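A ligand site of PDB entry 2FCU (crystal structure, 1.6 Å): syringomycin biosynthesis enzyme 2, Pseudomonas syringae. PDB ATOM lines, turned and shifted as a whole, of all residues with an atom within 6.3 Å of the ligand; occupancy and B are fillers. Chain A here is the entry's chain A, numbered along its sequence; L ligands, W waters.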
ATOM      1  N   GLU A 105     -13.665  -1.647 -24.778  1.00  0.00           N
ATOM      2  CA  GLU A 105     -14.467  -2.743 -24.276  1.00  0.00           C
ATOM      3  C   GLU A 105     -15.877  -2.696 -24.820  1.00  0.00           C
ATOM      4  O   GLU A 105     -16.550  -1.660 -24.725  1.00  0.00           O
ATOM      5  CB  GLU A 105     -14.467  -2.766 -22.738  1.00  0.00           C
ATOM      6  CG  GLU A 105     -15.208  -3.914 -22.077  1.00  0.00           C
ATOM      7  CD  GLU A 105     -15.033  -3.949 -20.559  1.00  0.00           C
ATOM      8  OE1 GLU A 105     -15.505  -4.927 -19.938  1.00  0.00           O
ATOM      9  OE2 GLU A 105     -14.438  -2.989 -20.011  1.00  0.00           O
ATOM     10  N   PHE A 107     -19.808  -3.760 -24.500  1.00  0.00           N
ATOM     11  CA  PHE A 107     -20.813  -4.072 -23.500  1.00  0.00           C
ATOM     12  C   PHE A 107     -22.128  -4.448 -24.160  1.00  0.00           C
ATOM     13  O   PHE A 107     -22.962  -3.603 -24.439  1.00  0.00           O
ATOM     14  CB  PHE A 107     -21.032  -2.887 -22.561  1.00  0.00           C
ATOM     15  CG  PHE A 107     -19.878  -2.656 -21.658  1.00  0.00           C
ATOM     16  CD1 PHE A 107     -18.876  -1.733 -21.984  1.00  0.00           C
ATOM     17  CD2 PHE A 107     -19.769  -3.365 -20.472  1.00  0.00           C
ATOM     18  CE1 PHE A 107     -17.810  -1.539 -21.154  1.00  0.00           C
ATOM     19  CE2 PHE A 107     -18.706  -3.153 -19.609  1.00  0.00           C
ATOM     20  CZ  PHE A 107     -17.721  -2.248 -19.958  1.00  0.00           C
ATOM     21  N   PRO A 108     -22.318  -5.747 -24.427  1.00  0.00           N
ATOM     22  CA  PRO A 108     -23.608  -6.192 -24.918  1.00  0.00           C
ATOM     23  C   PRO A 108     -24.621  -6.329 -23.795  1.00  0.00           C
ATOM     24  O   PRO A 108     -24.264  -6.765 -22.679  1.00  0.00           O
ATOM     25  CB  PRO A 108     -23.272  -7.574 -25.499  1.00  0.00           C
ATOM     26  CG  PRO A 108     -22.149  -8.082 -24.629  1.00  0.00           C
ATOM     27  CD  PRO A 108     -21.338  -6.837 -24.342  1.00  0.00           C
ATOM     28  N   LYS A 109     -25.863  -5.942 -24.073  1.00  0.00           N
ATOM     29  CA  LYS A 109     -26.993  -6.361 -23.207  1.00  0.00           C
ATOM     30  C   LYS A 109     -27.968  -7.097 -24.097  1.00  0.00           C
ATOM     31  O   LYS A 109     -28.598  -6.526 -24.969  1.00  0.00           O
ATOM     32  CB  LYS A 109     -27.715  -5.201 -22.505  1.00  0.00           C
ATOM     33  CG  LYS A 109     -26.900  -4.440 -21.516  1.00  0.00           C
ATOM     34  CD  LYS A 109     -26.676  -5.234 -20.238  1.00  0.00           C
ATOM     35  CE  LYS A 109     -25.941  -4.402 -19.231  1.00  0.00           C
ATOM     36  NZ  LYS A 109     -25.521  -5.184 -18.022  1.00  0.00           N
ATOM     37  N   GLY A 115     -29.050  -5.345 -15.284  1.00  0.00           N
ATOM     38  CA  GLY A 115     -28.310  -4.096 -15.325  1.00  0.00           C
ATOM     39  C   GLY A 115     -26.890  -4.235 -14.827  1.00  0.00           C
ATOM     40  O   GLY A 115     -26.589  -5.100 -13.976  1.00  0.00           O
ATOM     41  N   THR A 116     -26.006  -3.368 -15.312  1.00  0.00           N
ATOM     42  CA  THR A 116     -24.652  -3.340 -14.796  1.00  0.00           C
ATOM     43  C   THR A 116     -24.681  -2.775 -13.374  1.00  0.00           C
ATOM     44  O   THR A 116     -25.372  -1.795 -13.124  1.00  0.00           O
ATOM     45  CB  THR A 116     -23.728  -2.517 -15.702  1.00  0.00           C
ATOM     46  OG1 THR A 116     -23.778  -3.098 -17.012  1.00  0.00           O
ATOM     47  CG2 THR A 116     -22.288  -2.483 -15.164  1.00  0.00           C
ATOM     48  N   ASP A 117     -23.980  -3.416 -12.447  1.00  0.00           N
ATOM     49  CA  ASP A 117     -23.850  -2.934 -11.093  1.00  0.00           C
ATOM     50  C   ASP A 117     -23.353  -1.500 -11.029  1.00  0.00           C
ATOM     51  O   ASP A 117     -22.562  -1.049 -11.873  1.00  0.00           O
ATOM     52  CB  ASP A 117     -22.825  -3.761 -10.313  1.00  0.00           C
ATOM     53  CG  ASP A 117     -23.420  -5.005  -9.643  1.00  0.00           C
ATOM     54  OD1 ASP A 117     -24.633  -5.057  -9.351  1.00  0.00           O
ATOM     55  OD2 ASP A 117     -22.621  -5.932  -9.389  1.00  0.00           O
ATOM     56  N   HIS A 119     -20.790   1.047 -10.039  1.00  0.00           N
ATOM     57  CA  HIS A 119     -19.361   0.951  -9.871  1.00  0.00           C
ATOM     58  C   HIS A 119     -18.659   2.271 -10.166  1.00  0.00           C
ATOM     59  O   HIS A 119     -19.212   3.173 -10.803  1.00  0.00           O
ATOM     60  CB  HIS A 119     -18.784  -0.226 -10.678  1.00  0.00           C
ATOM     61  CG  HIS A 119     -18.898  -0.119 -12.159  1.00  0.00           C
ATOM     62  ND1 HIS A 119     -20.092  -0.097 -12.857  1.00  0.00           N
ATOM     63  CD2 HIS A 119     -17.912  -0.089 -13.103  1.00  0.00           C
ATOM     64  CE1 HIS A 119     -19.847  -0.020 -14.154  1.00  0.00           C
ATOM     65  NE2 HIS A 119     -18.539  -0.011 -14.328  1.00  0.00           N
ATOM     66  N   THR A 146     -13.817   7.757 -19.935  1.00  0.00           N
ATOM     67  CA  THR A 146     -14.545   6.800 -20.744  1.00  0.00           C
ATOM     68  C   THR A 146     -15.446   7.517 -21.740  1.00  0.00           C
ATOM     69  O   THR A 146     -16.174   8.447 -21.383  1.00  0.00           O
ATOM     70  CB  THR A 146     -15.385   5.863 -19.862  1.00  0.00           C
ATOM     71  OG1 THR A 146     -14.497   5.080 -19.075  1.00  0.00           O
ATOM     72  CG2 THR A 146     -16.292   4.933 -20.708  1.00  0.00           C
ATOM     73  N   TRP A 148     -18.327   6.273 -24.089  1.00  0.00           N
ATOM     74  CA  TRP A 148     -19.209   5.135 -24.334  1.00  0.00           C
ATOM     75  C   TRP A 148     -20.079   5.495 -25.537  1.00  0.00           C
ATOM     76  O   TRP A 148     -20.855   6.463 -25.502  1.00  0.00           O
ATOM     77  CB  TRP A 148     -20.052   4.882 -23.097  1.00  0.00           C
ATOM     78  CG  TRP A 148     -20.859   3.620 -23.031  1.00  0.00           C
ATOM     79  CD1 TRP A 148     -20.528   2.493 -22.345  1.00  0.00           C
ATOM     80  CD2 TRP A 148     -22.184   3.415 -23.532  1.00  0.00           C
ATOM     81  NE1 TRP A 148     -21.541   1.579 -22.434  1.00  0.00           N
ATOM     82  CE2 TRP A 148     -22.582   2.123 -23.137  1.00  0.00           C
ATOM     83  CE3 TRP A 148     -23.060   4.199 -24.257  1.00  0.00           C
ATOM     84  CZ2 TRP A 148     -23.844   1.599 -23.458  1.00  0.00           C
ATOM     85  CZ3 TRP A 148     -24.299   3.687 -24.593  1.00  0.00           C
ATOM     86  CH2 TRP A 148     -24.688   2.398 -24.180  1.00  0.00           C
ATOM     87  N   GLY A 159     -31.554  -1.163 -21.472  1.00  0.00           N
ATOM     88  CA  GLY A 159     -30.402  -1.121 -20.594  1.00  0.00           C
ATOM     89  C   GLY A 159     -29.445   0.029 -20.832  1.00  0.00           C
ATOM     90  O   GLY A 159     -28.220  -0.156 -20.784  1.00  0.00           O
ATOM     91  N   LEU A 161     -27.322   3.499 -19.974  1.00  0.00           N
ATOM     92  CA  LEU A 161     -26.544   3.891 -18.802  1.00  0.00           C
ATOM     93  C   LEU A 161     -27.332   4.784 -17.852  1.00  0.00           C
ATOM     94  O   LEU A 161     -28.311   5.421 -18.238  1.00  0.00           O
ATOM     95  CB  LEU A 161     -25.252   4.627 -19.201  1.00  0.00           C
ATOM     96  CG  LEU A 161     -24.285   3.791 -20.060  1.00  0.00           C
ATOM     97  CD1 LEU A 161     -22.993   4.594 -20.334  1.00  0.00           C
ATOM     98  CD2 LEU A 161     -23.940   2.462 -19.404  1.00  0.00           C
ATOM     99  N   PHE A 198     -22.422  -8.046 -12.221  1.00  0.00           N
ATOM    100  CA  PHE A 198     -21.144  -7.625 -12.800  1.00  0.00           C
ATOM    101  C   PHE A 198     -20.407  -8.858 -13.350  1.00  0.00           C
ATOM    102  O   PHE A 198     -19.423  -9.294 -12.795  1.00  0.00           O
ATOM    103  CB  PHE A 198     -20.328  -6.914 -11.746  1.00  0.00           C
ATOM    104  CG  PHE A 198     -19.259  -6.039 -12.303  1.00  0.00           C
ATOM    105  CD1 PHE A 198     -19.595  -4.803 -12.857  1.00  0.00           C
ATOM    106  CD2 PHE A 198     -17.913  -6.420 -12.273  1.00  0.00           C
ATOM    107  CE1 PHE A 198     -18.613  -3.963 -13.376  1.00  0.00           C
ATOM    108  CE2 PHE A 198     -16.930  -5.569 -12.782  1.00  0.00           C
ATOM    109  CZ  PHE A 198     -17.282  -4.352 -13.336  1.00  0.00           C
ATOM    110  N   PHE A 232     -17.490  10.419 -19.760  1.00  0.00           N
ATOM    111  CA  PHE A 232     -17.538  10.480 -18.291  1.00  0.00           C
ATOM    112  C   PHE A 232     -16.279   9.936 -17.655  1.00  0.00           C
ATOM    113  O   PHE A 232     -15.592   9.095 -18.233  1.00  0.00           O
ATOM    114  CB  PHE A 232     -18.781   9.755 -17.737  1.00  0.00           C
ATOM    115  CG  PHE A 232     -18.856   8.259 -18.054  1.00  0.00           C
ATOM    116  CD1 PHE A 232     -18.408   7.315 -17.139  1.00  0.00           C
ATOM    117  CD2 PHE A 232     -19.418   7.806 -19.224  1.00  0.00           C
ATOM    118  CE1 PHE A 232     -18.510   5.948 -17.407  1.00  0.00           C
ATOM    119  CE2 PHE A 232     -19.528   6.446 -19.500  1.00  0.00           C
ATOM    120  CZ  PHE A 232     -19.046   5.520 -18.595  1.00  0.00           C
ATOM    121  N   SER A 234     -14.337   7.532 -15.278  1.00  0.00           N
ATOM    122  CA  SER A 234     -14.582   6.158 -14.744  1.00  0.00           C
ATOM    123  C   SER A 234     -14.821   6.144 -13.232  1.00  0.00           C
ATOM    124  O   SER A 234     -15.355   5.175 -12.684  1.00  0.00           O
ATOM    125  CB  SER A 234     -13.396   5.241 -15.100  1.00  0.00           C
ATOM    126  OG  SER A 234     -12.218   5.721 -14.488  1.00  0.00           O
ATOM    127  N   HIS A 238     -21.549   4.967 -11.864  1.00  0.00           N
ATOM    128  CA  HIS A 238     -22.282   4.613 -13.077  1.00  0.00           C
ATOM    129  C   HIS A 238     -22.728   3.162 -13.052  1.00  0.00           C
ATOM    130  O   HIS A 238     -22.167   2.338 -12.352  1.00  0.00           O
ATOM    131  CB  HIS A 238     -21.492   4.968 -14.372  1.00  0.00           C
ATOM    132  CG  HIS A 238     -20.184   4.250 -14.538  1.00  0.00           C
ATOM    133  ND1 HIS A 238     -19.065   4.522 -13.784  1.00  0.00           N
ATOM    134  CD2 HIS A 238     -19.798   3.324 -15.459  1.00  0.00           C
ATOM    135  CE1 HIS A 238     -18.056   3.779 -14.191  1.00  0.00           C
ATOM    136  NE2 HIS A 238     -18.483   3.020 -15.198  1.00  0.00           N
ATOM    137  N   ALA A 239     -23.783   2.912 -13.809  1.00  0.00           N
ATOM    138  CA  ALA A 239     -24.436   1.623 -13.852  1.00  0.00           C
ATOM    139  C   ALA A 239     -25.237   1.555 -15.156  1.00  0.00           C
ATOM    140  O   ALA A 239     -25.166   2.465 -15.968  1.00  0.00           O
ATOM    141  CB  ALA A 239     -25.353   1.491 -12.631  1.00  0.00           C
ATOM    142  N   SER A 240     -26.002   0.505 -15.362  1.00  0.00           N
ATOM    143  CA  SER A 240     -26.994   0.512 -16.422  1.00  0.00           C
ATOM    144  C   SER A 240     -28.293  -0.091 -15.916  1.00  0.00           C
ATOM    145  O   SER A 240     -28.331  -0.887 -14.947  1.00  0.00           O
ATOM    146  CB  SER A 240     -26.559  -0.249 -17.667  1.00  0.00           C
ATOM    147  OG  SER A 240     -26.921  -1.621 -17.561  1.00  0.00           O
ATOM    148  N   ARG A 251     -28.816  -4.555 -27.012  1.00  0.00           N
ATOM    149  CA  ARG A 251     -28.140  -3.271 -26.913  1.00  0.00           C
ATOM    150  C   ARG A 251     -26.641  -3.490 -26.976  1.00  0.00           C
ATOM    151  O   ARG A 251     -26.114  -4.455 -26.395  1.00  0.00           O
ATOM    152  CB  ARG A 251     -28.476  -2.613 -25.576  1.00  0.00           C
ATOM    153  CG  ARG A 251     -27.754  -1.301 -25.289  1.00  0.00           C
ATOM    154  CD  ARG A 251     -26.420  -1.514 -24.553  1.00  0.00           C
ATOM    155  NE  ARG A 251     -26.561  -1.418 -23.121  1.00  0.00           N
ATOM    156  CZ  ARG A 251     -25.572  -1.501 -22.240  1.00  0.00           C
ATOM    157  NH1 ARG A 251     -24.328  -1.830 -22.609  1.00  0.00           N
ATOM    158  NH2 ARG A 251     -25.800  -1.289 -20.954  1.00  0.00           N
ATOM    159  N   GLY A 253     -23.038  -1.247 -26.392  1.00  0.00           N
ATOM    160  CA  GLY A 253     -22.210  -0.069 -26.137  1.00  0.00           C
ATOM    161  C   GLY A 253     -20.776  -0.434 -26.438  1.00  0.00           C
ATOM    162  O   GLY A 253     -20.349  -1.582 -26.252  1.00  0.00           O
ATOM    163  N   ALA A 255     -17.085   1.088 -25.291  1.00  0.00           N
ATOM    164  CA  ALA A 255     -16.320   2.004 -24.437  1.00  0.00           C
ATOM    165  C   ALA A 255     -14.905   2.108 -24.966  1.00  0.00           C
ATOM    166  O   ALA A 255     -14.234   1.070 -25.173  1.00  0.00           O
ATOM    167  CB  ALA A 255     -16.265   1.543 -22.947  1.00  0.00           C
ATOM    168  N   ARG A 257     -11.334   4.096 -23.686  1.00  0.00           N
ATOM    169  CA  ARG A 257     -10.817   4.666 -22.443  1.00  0.00           C
ATOM    170  C   ARG A 257      -9.502   5.413 -22.708  1.00  0.00           C
ATOM    171  O   ARG A 257      -8.625   4.898 -23.404  1.00  0.00           O
ATOM    172  CB  ARG A 257     -10.655   3.601 -21.362  1.00  0.00           C
ATOM    173  CG  ARG A 257     -11.924   2.748 -21.160  1.00  0.00           C
ATOM    174  CD  ARG A 257     -11.916   1.999 -19.836  1.00  0.00           C
ATOM    175  NE  ARG A 257     -12.895   0.901 -19.799  1.00  0.00           N
ATOM    176  CZ  ARG A 257     -14.223   1.048 -19.732  1.00  0.00           C
ATOM    177  NH1 ARG A 257     -15.014  -0.014 -19.695  1.00  0.00           N
ATOM    178  NH2 ARG A 257     -14.789   2.246 -19.741  1.00  0.00           N
HETATM  179  C1  LIG L   1     -18.178   1.546 -18.623  1.00  0.00           C
HETATM  180  O1  LIG L   1     -17.837   1.626 -19.800  1.00  0.00           O
HETATM  181  O2  LIG L   1     -17.558   2.141 -17.721  1.00  0.00           O
HETATM  182  C2  LIG L   1     -19.372   0.793 -18.248  1.00  0.00           C
HETATM  183  O3  LIG L   1     -19.459   0.470 -17.082  1.00  0.00           O
HETATM  184  C3  LIG L   1     -20.461   0.445 -19.234  1.00  0.00           C
HETATM  185  C4  LIG L   1     -21.512  -0.525 -18.647  1.00  0.00           C
HETATM  186  C5  LIG L   1     -22.569  -0.957 -19.635  1.00  0.00           C
HETATM  187  O4  LIG L   1     -22.451  -0.681 -20.855  1.00  0.00           O
HETATM  188  O5  LIG L   1     -23.557  -1.606 -19.167  1.00  0.00           O
HETATM  189  O   HOH W   1     -16.626  -0.682 -16.371  1.00  0.00           O
HETATM  190  O   HOH W   2     -15.341   1.815 -15.602  1.00  0.00           O
HETATM  191  O   HOH W   3     -15.675   3.880 -16.942  1.00  0.00           O
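An oxygen (O5) of the ligand sits at hydrogen-bond distance from the side-chain hydroxyl of Thr 116, 2.6 Å away.
O3 of the ligand sits at hydrogen-bond distance from NE2 of His 119 (2.9 Å).
The indole nitrogen of Trp 148 is in hydrogen-bond range of an oxygen (O4) of the ligand (2.9 Å).
The guanidinium group (NH1) of Arg 251 lies within salt-bridge range of an oxygen (O4) of the ligand (2.8 Å).
NE2 of His 238 lies within hydrogen-bond range of O2 of the ligand (2.8 Å).
An oxygen (O1) of the ligand is in salt-bridge range of the guanidinium group (NH2) of Arg 257, at 3.1 Å.
NH2 of Arg 257 lies within hydrogen-bond range of OG1 of Thr 146 (2.9 Å).
The backbone carbonyl oxygen (O) of Gly 253 lies within hydrogen-bond range of the backbone NH (N) of Phe 107, at 2.8 Å.
The side-chain carboxylate (OE2) of Glu 105 lies within salt-bridge range of the guanidinium group (NH1) of Arg 257, 3.0 Å away.
NH2 of Arg 251 is in hydrogen-bond range of O of Gly 159.
The backbone NH (N) of Thr 116 is in hydrogen-bond range of the side-chain hydroxyl (OG) of Ser 240 (3.0 Å).
OG1 of Thr 116 lies within hydrogen-bond range of NZ of Lys 109, at 2.9 Å.
The guanidinium group of Arg 251 lies within hydrogen-bond range of the backbone carbonyl oxygen of Phe 107, 2.9 Å away.
The backbone NH (N) of Thr 146 lies within hydrogen-bond range of the backbone carbonyl oxygen (O) of Phe 232 (2.8 Å).
CB of Phe 107 touches O4 of the ligand (3.1 Å).
Lys 109 touches the ligand.
Thr 146 touches the ligand.
Leu 161 touches the ligand.
Phe 232 touches the ligand (CZ to O2, 3.8 Å).
Ser 240 touches the ligand.
CB of Ala 255 touches O1 of the ligand (3.5 Å).
Hydrophobic or aromatic side chains within 4 Å of the ligand: Phe 107, His 119, Trp 148, Leu 161, Phe 232, His 238 and Ala 255.
Of the 22 residues printed, 13 come within 4 Å of the ligand.
Water W3 lies within hydrogen-bond range of O2 of the ligand (2.7 Å), OG1 of Thr 146 (2.7 Å), NH2 of Arg 257 (3.4 Å) and NE2 of His 238 (3.4 Å).
Water W2 bridges an oxygen (O2) of the ligand and a ring nitrogen (NE2) of His 238.
Water W1 lies within hydrogen-bond range of a ring nitrogen (NE2) of His 119 (2.9 Å) and an oxygen (O3) of the ligand (3.1 Å).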
